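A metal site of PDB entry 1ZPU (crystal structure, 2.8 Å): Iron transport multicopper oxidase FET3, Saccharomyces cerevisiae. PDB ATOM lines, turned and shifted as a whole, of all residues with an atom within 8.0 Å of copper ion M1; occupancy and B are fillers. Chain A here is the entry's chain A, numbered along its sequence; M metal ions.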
ATOM      1  N   HIS A  60       5.770 -11.368  21.981  1.00  0.00           N
ATOM      2  CA  HIS A  60       6.100 -11.955  23.263  1.00  0.00           C
ATOM      3  C   HIS A  60       7.269 -12.898  23.075  1.00  0.00           C
ATOM      4  O   HIS A  60       7.315 -13.651  22.112  1.00  0.00           O
ATOM      5  CB  HIS A  60       4.898 -12.720  23.791  1.00  0.00           C
ATOM      6  CG  HIS A  60       5.222 -13.646  24.929  1.00  0.00           C
ATOM      7  ND1 HIS A  60       5.902 -13.239  26.050  1.00  0.00           N
ATOM      8  CD2 HIS A  60       4.929 -14.954  25.119  1.00  0.00           C
ATOM      9  CE1 HIS A  60       6.037 -14.251  26.877  1.00  0.00           C
ATOM     10  NE2 HIS A  60       5.452 -15.300  26.336  1.00  0.00           N
ATOM     11  N   PHE A  61       8.211 -12.872  24.017  1.00  0.00           N
ATOM     12  CA  PHE A  61       9.376 -13.749  23.962  1.00  0.00           C
ATOM     13  C   PHE A  61       9.225 -14.877  24.976  1.00  0.00           C
ATOM     14  O   PHE A  61       9.471 -14.708  26.162  1.00  0.00           O
ATOM     15  CB  PHE A  61      10.641 -12.931  24.124  1.00  0.00           C
ATOM     16  CG  PHE A  61      10.691 -11.765  23.199  1.00  0.00           C
ATOM     17  CD1 PHE A  61      10.093 -10.544  23.572  1.00  0.00           C
ATOM     18  CD2 PHE A  61      11.247 -11.889  21.935  1.00  0.00           C
ATOM     19  CE1 PHE A  61      10.088  -9.470  22.706  1.00  0.00           C
ATOM     20  CE2 PHE A  61      11.245 -10.816  21.055  1.00  0.00           C
ATOM     21  CZ  PHE A  61      10.672  -9.603  21.442  1.00  0.00           C
ATOM     22  N   HIS A  62       8.794 -16.028  24.465  1.00  0.00           N
ATOM     23  CA  HIS A  62       8.293 -17.118  25.268  1.00  0.00           C
ATOM     24  C   HIS A  62       9.367 -17.738  26.121  1.00  0.00           C
ATOM     25  O   HIS A  62      10.332 -18.312  25.594  1.00  0.00           O
ATOM     26  CB  HIS A  62       7.703 -18.201  24.363  1.00  0.00           C
ATOM     27  CG  HIS A  62       7.015 -19.296  25.113  1.00  0.00           C
ATOM     28  ND1 HIS A  62       5.664 -19.531  25.005  1.00  0.00           N
ATOM     29  CD2 HIS A  62       7.493 -20.212  25.988  1.00  0.00           C
ATOM     30  CE1 HIS A  62       5.338 -20.547  25.787  1.00  0.00           C
ATOM     31  NE2 HIS A  62       6.432 -20.968  26.396  1.00  0.00           N
ATOM     32  N   GLY A  63       9.198 -17.655  27.430  1.00  0.00           N
ATOM     33  CA  GLY A  63      10.066 -18.376  28.357  1.00  0.00           C
ATOM     34  C   GLY A  63      11.020 -17.452  29.077  1.00  0.00           C
ATOM     35  O   GLY A  63      11.514 -17.781  30.155  1.00  0.00           O
ATOM     36  N   TRP A 103      11.427 -19.217  21.986  1.00  0.00           N
ATOM     37  CA  TRP A 103      10.880 -18.650  20.762  1.00  0.00           C
ATOM     38  C   TRP A 103      10.093 -17.377  21.033  1.00  0.00           C
ATOM     39  O   TRP A 103       9.768 -17.037  22.185  1.00  0.00           O
ATOM     40  CB  TRP A 103      10.017 -19.662  20.004  1.00  0.00           C
ATOM     41  CG  TRP A 103       8.789 -20.180  20.735  1.00  0.00           C
ATOM     42  CD1 TRP A 103       8.773 -20.839  21.923  1.00  0.00           C
ATOM     43  CD2 TRP A 103       7.427 -20.141  20.269  1.00  0.00           C
ATOM     44  NE1 TRP A 103       7.485 -21.178  22.254  1.00  0.00           N
ATOM     45  CE2 TRP A 103       6.645 -20.767  21.262  1.00  0.00           C
ATOM     46  CE3 TRP A 103       6.810 -19.634  19.134  1.00  0.00           C
ATOM     47  CZ2 TRP A 103       5.258 -20.889  21.137  1.00  0.00           C
ATOM     48  CZ3 TRP A 103       5.427 -19.764  19.012  1.00  0.00           C
ATOM     49  CH2 TRP A 103       4.674 -20.388  20.011  1.00  0.00           C
ATOM     50  N   TYR A 104       9.818 -16.649  19.966  1.00  0.00           N
ATOM     51  CA  TYR A 104       9.020 -15.457  20.059  1.00  0.00           C
ATOM     52  C   TYR A 104       7.824 -15.581  19.142  1.00  0.00           C
ATOM     53  O   TYR A 104       7.907 -16.161  18.058  1.00  0.00           O
ATOM     54  CB  TYR A 104       9.878 -14.250  19.692  1.00  0.00           C
ATOM     55  CG  TYR A 104      10.264 -14.140  18.239  1.00  0.00           C
ATOM     56  CD1 TYR A 104       9.458 -13.451  17.352  1.00  0.00           C
ATOM     57  CD2 TYR A 104      11.452 -14.704  17.766  1.00  0.00           C
ATOM     58  CE1 TYR A 104       9.814 -13.332  16.022  1.00  0.00           C
ATOM     59  CE2 TYR A 104      11.819 -14.592  16.432  1.00  0.00           C
ATOM     60  CZ  TYR A 104      10.994 -13.898  15.554  1.00  0.00           C
ATOM     61  OH  TYR A 104      11.338 -13.760  14.235  1.00  0.00           O
ATOM     62  N   HIS A 105       6.694 -15.033  19.565  1.00  0.00           N
ATOM     63  CA  HIS A 105       5.493 -15.029  18.754  1.00  0.00           C
ATOM     64  C   HIS A 105       4.658 -13.803  19.062  1.00  0.00           C
ATOM     65  O   HIS A 105       4.783 -13.220  20.137  1.00  0.00           O
ATOM     66  CB  HIS A 105       4.652 -16.296  18.990  1.00  0.00           C
ATOM     67  CG  HIS A 105       4.251 -16.528  20.419  1.00  0.00           C
ATOM     68  ND1 HIS A 105       3.146 -15.931  20.991  1.00  0.00           N
ATOM     69  CD2 HIS A 105       4.802 -17.306  21.390  1.00  0.00           C
ATOM     70  CE1 HIS A 105       3.040 -16.318  22.247  1.00  0.00           C
ATOM     71  NE2 HIS A 105       4.027 -17.149  22.518  1.00  0.00           N
ATOM     72  N   SER A 106       3.824 -13.405  18.108  1.00  0.00           N
ATOM     73  CA  SER A 106       2.827 -12.376  18.346  1.00  0.00           C
ATOM     74  C   SER A 106       1.911 -12.830  19.461  1.00  0.00           C
ATOM     75  O   SER A 106       1.586 -14.013  19.555  1.00  0.00           O
ATOM     76  CB  SER A 106       2.015 -12.136  17.081  1.00  0.00           C
ATOM     77  OG  SER A 106       0.867 -11.349  17.336  1.00  0.00           O
ATOM     78  N   HIS A 107       1.502 -11.913  20.325  1.00  0.00           N
ATOM     79  CA  HIS A 107       0.539 -12.256  21.370  1.00  0.00           C
ATOM     80  C   HIS A 107      -0.828 -11.586  21.150  1.00  0.00           C
ATOM     81  O   HIS A 107      -1.631 -11.500  22.079  1.00  0.00           O
ATOM     82  CB  HIS A 107       1.097 -11.923  22.751  1.00  0.00           C
ATOM     83  CG  HIS A 107       0.761 -12.950  23.801  1.00  0.00           C
ATOM     84  ND1 HIS A 107      -0.475 -13.005  24.408  1.00  0.00           N
ATOM     85  CD2 HIS A 107       1.493 -13.959  24.328  1.00  0.00           C
ATOM     86  CE1 HIS A 107      -0.485 -13.997  25.272  1.00  0.00           C
ATOM     87  NE2 HIS A 107       0.693 -14.597  25.237  1.00  0.00           N
ATOM     88  N   TYR A 112      -0.033 -15.214  15.504  1.00  0.00           N
ATOM     89  CA  TYR A 112       1.147 -16.081  15.277  1.00  0.00           C
ATOM     90  C   TYR A 112       0.920 -17.330  14.400  1.00  0.00           C
ATOM     91  O   TYR A 112       1.828 -17.740  13.687  1.00  0.00           O
ATOM     92  CB  TYR A 112       1.991 -16.378  16.525  1.00  0.00           C
ATOM     93  CG  TYR A 112       1.628 -17.588  17.363  1.00  0.00           C
ATOM     94  CD1 TYR A 112       2.026 -18.884  17.012  1.00  0.00           C
ATOM     95  CD2 TYR A 112       0.951 -17.419  18.564  1.00  0.00           C
ATOM     96  CE1 TYR A 112       1.721 -19.973  17.826  1.00  0.00           C
ATOM     97  CE2 TYR A 112       0.639 -18.477  19.381  1.00  0.00           C
ATOM     98  CZ  TYR A 112       1.020 -19.749  19.018  1.00  0.00           C
ATOM     99  OH  TYR A 112       0.666 -20.774  19.881  1.00  0.00           O
ATOM    100  N   ASN A 194       7.711 -26.990  19.209  1.00  0.00           N
ATOM    101  CA  ASN A 194       6.369 -26.895  18.635  1.00  0.00           C
ATOM    102  C   ASN A 194       5.827 -25.450  18.634  1.00  0.00           C
ATOM    103  O   ASN A 194       5.305 -24.970  19.639  1.00  0.00           O
ATOM    104  CB  ASN A 194       5.411 -27.872  19.289  1.00  0.00           C
ATOM    105  CG  ASN A 194       4.082 -27.883  18.595  1.00  0.00           C
ATOM    106  OD1 ASN A 194       3.795 -26.967  17.796  1.00  0.00           O
ATOM    107  ND2 ASN A 194       3.266 -28.888  18.862  1.00  0.00           N
ATOM    108  N   GLY A 196       3.341 -24.346  17.016  1.00  0.00           N
ATOM    109  CA  GLY A 196       1.980 -24.404  16.507  1.00  0.00           C
ATOM    110  C   GLY A 196       1.021 -23.610  17.376  1.00  0.00           C
ATOM    111  O   GLY A 196       1.390 -23.138  18.461  1.00  0.00           O
ATOM    112  N   VAL A 232       1.980 -27.548  21.911  1.00  0.00           N
ATOM    113  CA  VAL A 232       2.403 -26.262  21.338  1.00  0.00           C
ATOM    114  C   VAL A 232       3.147 -25.503  22.406  1.00  0.00           C
ATOM    115  O   VAL A 232       2.837 -25.638  23.595  1.00  0.00           O
ATOM    116  CB  VAL A 232       1.250 -25.446  20.788  1.00  0.00           C
ATOM    117  CG1 VAL A 232       0.573 -26.202  19.692  1.00  0.00           C
ATOM    118  CG2 VAL A 232       0.262 -25.094  21.865  1.00  0.00           C
ATOM    119  N   ALA A 233       4.151 -24.740  21.990  1.00  0.00           N
ATOM    120  CA  ALA A 233       4.904 -23.854  22.876  1.00  0.00           C
ATOM    121  C   ALA A 233       6.021 -24.538  23.634  1.00  0.00           C
ATOM    122  O   ALA A 233       6.910 -23.870  24.146  1.00  0.00           O
ATOM    123  CB  ALA A 233       3.970 -23.120  23.843  1.00  0.00           C
ATOM    124  N   GLN A 234       6.010 -25.858  23.733  1.00  0.00           N
ATOM    125  CA  GLN A 234       7.113 -26.503  24.435  1.00  0.00           C
ATOM    126  C   GLN A 234       8.302 -26.842  23.545  1.00  0.00           C
ATOM    127  O   GLN A 234       8.153 -26.951  22.327  1.00  0.00           O
ATOM    128  CB  GLN A 234       6.704 -27.636  25.386  1.00  0.00           C
ATOM    129  CG  GLN A 234       5.790 -28.743  24.908  1.00  0.00           C
ATOM    130  CD  GLN A 234       5.219 -29.573  26.090  1.00  0.00           C
ATOM    131  OE1 GLN A 234       4.980 -29.047  27.198  1.00  0.00           O
ATOM    132  NE2 GLN A 234       4.989 -30.875  25.850  1.00  0.00           N
ATOM    133  N   ARG A 235       9.470 -26.974  24.159  1.00  0.00           N
ATOM    134  CA  ARG A 235      10.703 -27.270  23.459  1.00  0.00           C
ATOM    135  C   ARG A 235      11.343 -28.493  24.081  1.00  0.00           C
ATOM    136  O   ARG A 235      11.497 -28.559  25.298  1.00  0.00           O
ATOM    137  CB  ARG A 235      11.678 -26.088  23.590  1.00  0.00           C
ATOM    138  CG  ARG A 235      11.246 -24.845  22.878  1.00  0.00           C
ATOM    139  CD  ARG A 235      10.252 -24.013  23.678  1.00  0.00           C
ATOM    140  NE  ARG A 235      10.902 -23.253  24.737  1.00  0.00           N
ATOM    141  CZ  ARG A 235      10.357 -22.909  25.900  1.00  0.00           C
ATOM    142  NH1 ARG A 235       9.110 -23.262  26.177  1.00  0.00           N
ATOM    143  NH2 ARG A 235      11.057 -22.234  26.795  1.00  0.00           N
ATOM    144  N   HIS A 395       0.593 -22.502  30.046  1.00  0.00           N
ATOM    145  CA  HIS A 395       1.885 -21.871  30.089  1.00  0.00           C
ATOM    146  C   HIS A 395       1.855 -20.697  31.070  1.00  0.00           C
ATOM    147  O   HIS A 395       0.829 -20.003  31.187  1.00  0.00           O
ATOM    148  CB  HIS A 395       2.307 -21.459  28.682  1.00  0.00           C
ATOM    149  CG  HIS A 395       3.385 -20.425  28.658  1.00  0.00           C
ATOM    150  ND1 HIS A 395       4.658 -20.660  29.123  1.00  0.00           N
ATOM    151  CD2 HIS A 395       3.367 -19.141  28.248  1.00  0.00           C
ATOM    152  CE1 HIS A 395       5.379 -19.571  28.995  1.00  0.00           C
ATOM    153  NE2 HIS A 395       4.618 -18.631  28.465  1.00  0.00           N
ATOM    154  N   HIS A 397       3.888 -17.228  32.265  1.00  0.00           N
ATOM    155  CA  HIS A 397       4.878 -16.193  31.972  1.00  0.00           C
ATOM    156  C   HIS A 397       5.746 -15.926  33.207  1.00  0.00           C
ATOM    157  O   HIS A 397       5.289 -16.127  34.336  1.00  0.00           O
ATOM    158  CB  HIS A 397       4.202 -14.892  31.569  1.00  0.00           C
ATOM    159  CG  HIS A 397       3.617 -14.924  30.196  1.00  0.00           C
ATOM    160  ND1 HIS A 397       3.892 -13.962  29.245  1.00  0.00           N
ATOM    161  CD2 HIS A 397       2.738 -15.779  29.612  1.00  0.00           C
ATOM    162  CE1 HIS A 397       3.219 -14.229  28.145  1.00  0.00           C
ATOM    163  NE2 HIS A 397       2.516 -15.332  28.330  1.00  0.00           N
ATOM    164  N   ASP A 437       8.086 -24.385  31.479  1.00  0.00           N
ATOM    165  CA  ASP A 437       7.176 -23.251  31.402  1.00  0.00           C
ATOM    166  C   ASP A 437       5.832 -23.590  30.772  1.00  0.00           C
ATOM    167  O   ASP A 437       4.902 -22.790  30.802  1.00  0.00           O
ATOM    168  CB  ASP A 437       7.838 -22.034  30.725  1.00  0.00           C
ATOM    169  CG  ASP A 437       8.205 -22.285  29.279  1.00  0.00           C
ATOM    170  OD1 ASP A 437       9.382 -21.996  28.946  1.00  0.00           O
ATOM    171  OD2 ASP A 437       7.350 -22.755  28.491  1.00  0.00           O
ATOM    172  N   THR A 438       5.714 -24.795  30.231  1.00  0.00           N
ATOM    173  CA  THR A 438       4.502 -25.184  29.548  1.00  0.00           C
ATOM    174  C   THR A 438       4.256 -26.655  29.820  1.00  0.00           C
ATOM    175  O   THR A 438       5.136 -27.482  29.634  1.00  0.00           O
ATOM    176  CB  THR A 438       4.609 -24.866  28.027  1.00  0.00           C
ATOM    177  OG1 THR A 438       5.039 -23.505  27.859  1.00  0.00           O
ATOM    178  CG2 THR A 438       3.283 -25.089  27.312  1.00  0.00           C
ATOM    179  N   HIS A 462      -2.197 -19.081  31.129  1.00  0.00           N
ATOM    180  CA  HIS A 462      -3.240 -19.442  30.179  1.00  0.00           C
ATOM    181  C   HIS A 462      -2.925 -20.696  29.404  1.00  0.00           C
ATOM    182  O   HIS A 462      -1.785 -21.168  29.372  1.00  0.00           O
ATOM    183  CB  HIS A 462      -3.435 -18.311  29.175  1.00  0.00           C
ATOM    184  CG  HIS A 462      -2.244 -18.081  28.296  1.00  0.00           C
ATOM    185  ND1 HIS A 462      -2.082 -18.716  27.082  1.00  0.00           N
ATOM    186  CD2 HIS A 462      -1.151 -17.306  28.462  1.00  0.00           C
ATOM    187  CE1 HIS A 462      -0.944 -18.339  26.536  1.00  0.00           C
ATOM    188  NE2 HIS A 462      -0.351 -17.492  27.357  1.00  0.00           N
ATOM    189  N   HIS A 464      -2.173 -22.352  25.934  1.00  0.00           N
ATOM    190  CA  HIS A 464      -1.456 -21.884  24.777  1.00  0.00           C
ATOM    191  C   HIS A 464      -2.094 -22.300  23.440  1.00  0.00           C
ATOM    192  O   HIS A 464      -1.546 -22.035  22.380  1.00  0.00           O
ATOM    193  CB  HIS A 464      -0.004 -22.312  24.832  1.00  0.00           C
ATOM    194  CG  HIS A 464       0.934 -21.308  24.252  1.00  0.00           C
ATOM    195  ND1 HIS A 464       1.019 -21.082  22.892  1.00  0.00           N
ATOM    196  CD2 HIS A 464       1.813 -20.454  24.835  1.00  0.00           C
ATOM    197  CE1 HIS A 464       1.906 -20.126  22.667  1.00  0.00           C
ATOM    198  NE2 HIS A 464       2.408 -19.735  23.834  1.00  0.00           N
ATOM    199  N   GLU A 466      -4.335 -21.368  20.815  1.00  0.00           N
ATOM    200  CA  GLU A 466      -4.789 -20.053  20.428  1.00  0.00           C
ATOM    201  C   GLU A 466      -6.305 -19.880  20.470  1.00  0.00           C
ATOM    202  O   GLU A 466      -6.813 -18.833  20.891  1.00  0.00           O
ATOM    203  CB  GLU A 466      -4.223 -19.724  19.061  1.00  0.00           C
ATOM    204  CG  GLU A 466      -2.806 -19.161  19.161  1.00  0.00           C
ATOM    205  CD  GLU A 466      -2.793 -17.701  19.651  1.00  0.00           C
ATOM    206  OE1 GLU A 466      -3.259 -16.818  18.869  1.00  0.00           O
ATOM    207  OE2 GLU A 466      -2.343 -17.458  20.801  1.00  0.00           O
HETATM  208 CU    CU M   1       4.304 -18.569  23.993  1.00  0.00          CU
HETATM  209 CU    CU M   2       5.438 -16.983  27.562  1.00  0.00          CU
HETATM  210 CU    CU M   3       1.063 -15.859  26.862  1.00  0.00          CU
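The backbone carbonyl oxygen (O) of His 105 lies within hydrogen-bond range of the backbone NH (N) of His 60 (2.8 Å).
ND1 of His 395 lies close to NE2 of His 62 (3.3 Å).
The indole nitrogen (NE1) of Trp 103 sits at hydrogen-bond distance from the backbone carbonyl oxygen (O) of Ala 233 (3.3 Å).
A ring nitrogen (ND1) of His 464 lies within hydrogen-bond range of the side-chain hydroxyl (OH) of Tyr 112 (3.0 Å).
NE2 of His 62 sits at hydrogen-bond distance from OG1 of Thr 438 (3.2 Å).
A ring nitrogen (NE2) of His 62 sits at hydrogen-bond distance from the side-chain carboxylate of Asp 437, 2.9 Å away.
The backbone NH (N) of His 62 is in hydrogen-bond range of the backbone carbonyl oxygen (O) of Trp 103, 2.7 Å away.
His 60 touches copper ion M1.
CZ2 of Trp 103 touches copper ion M1, at 3.8 Å.
Within 4 Å of copper ion M1: His 60, His 62, Trp 103, His 105 and His 464.
ND1 of His 62 binds copper ion M1, 1.9 Å away.
NE2 of His 105 is bound to copper ion M1, 2.1 Å away.
Copper ion M1 is bound by a ring nitrogen (NE2) of His 464 (2.2 Å).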
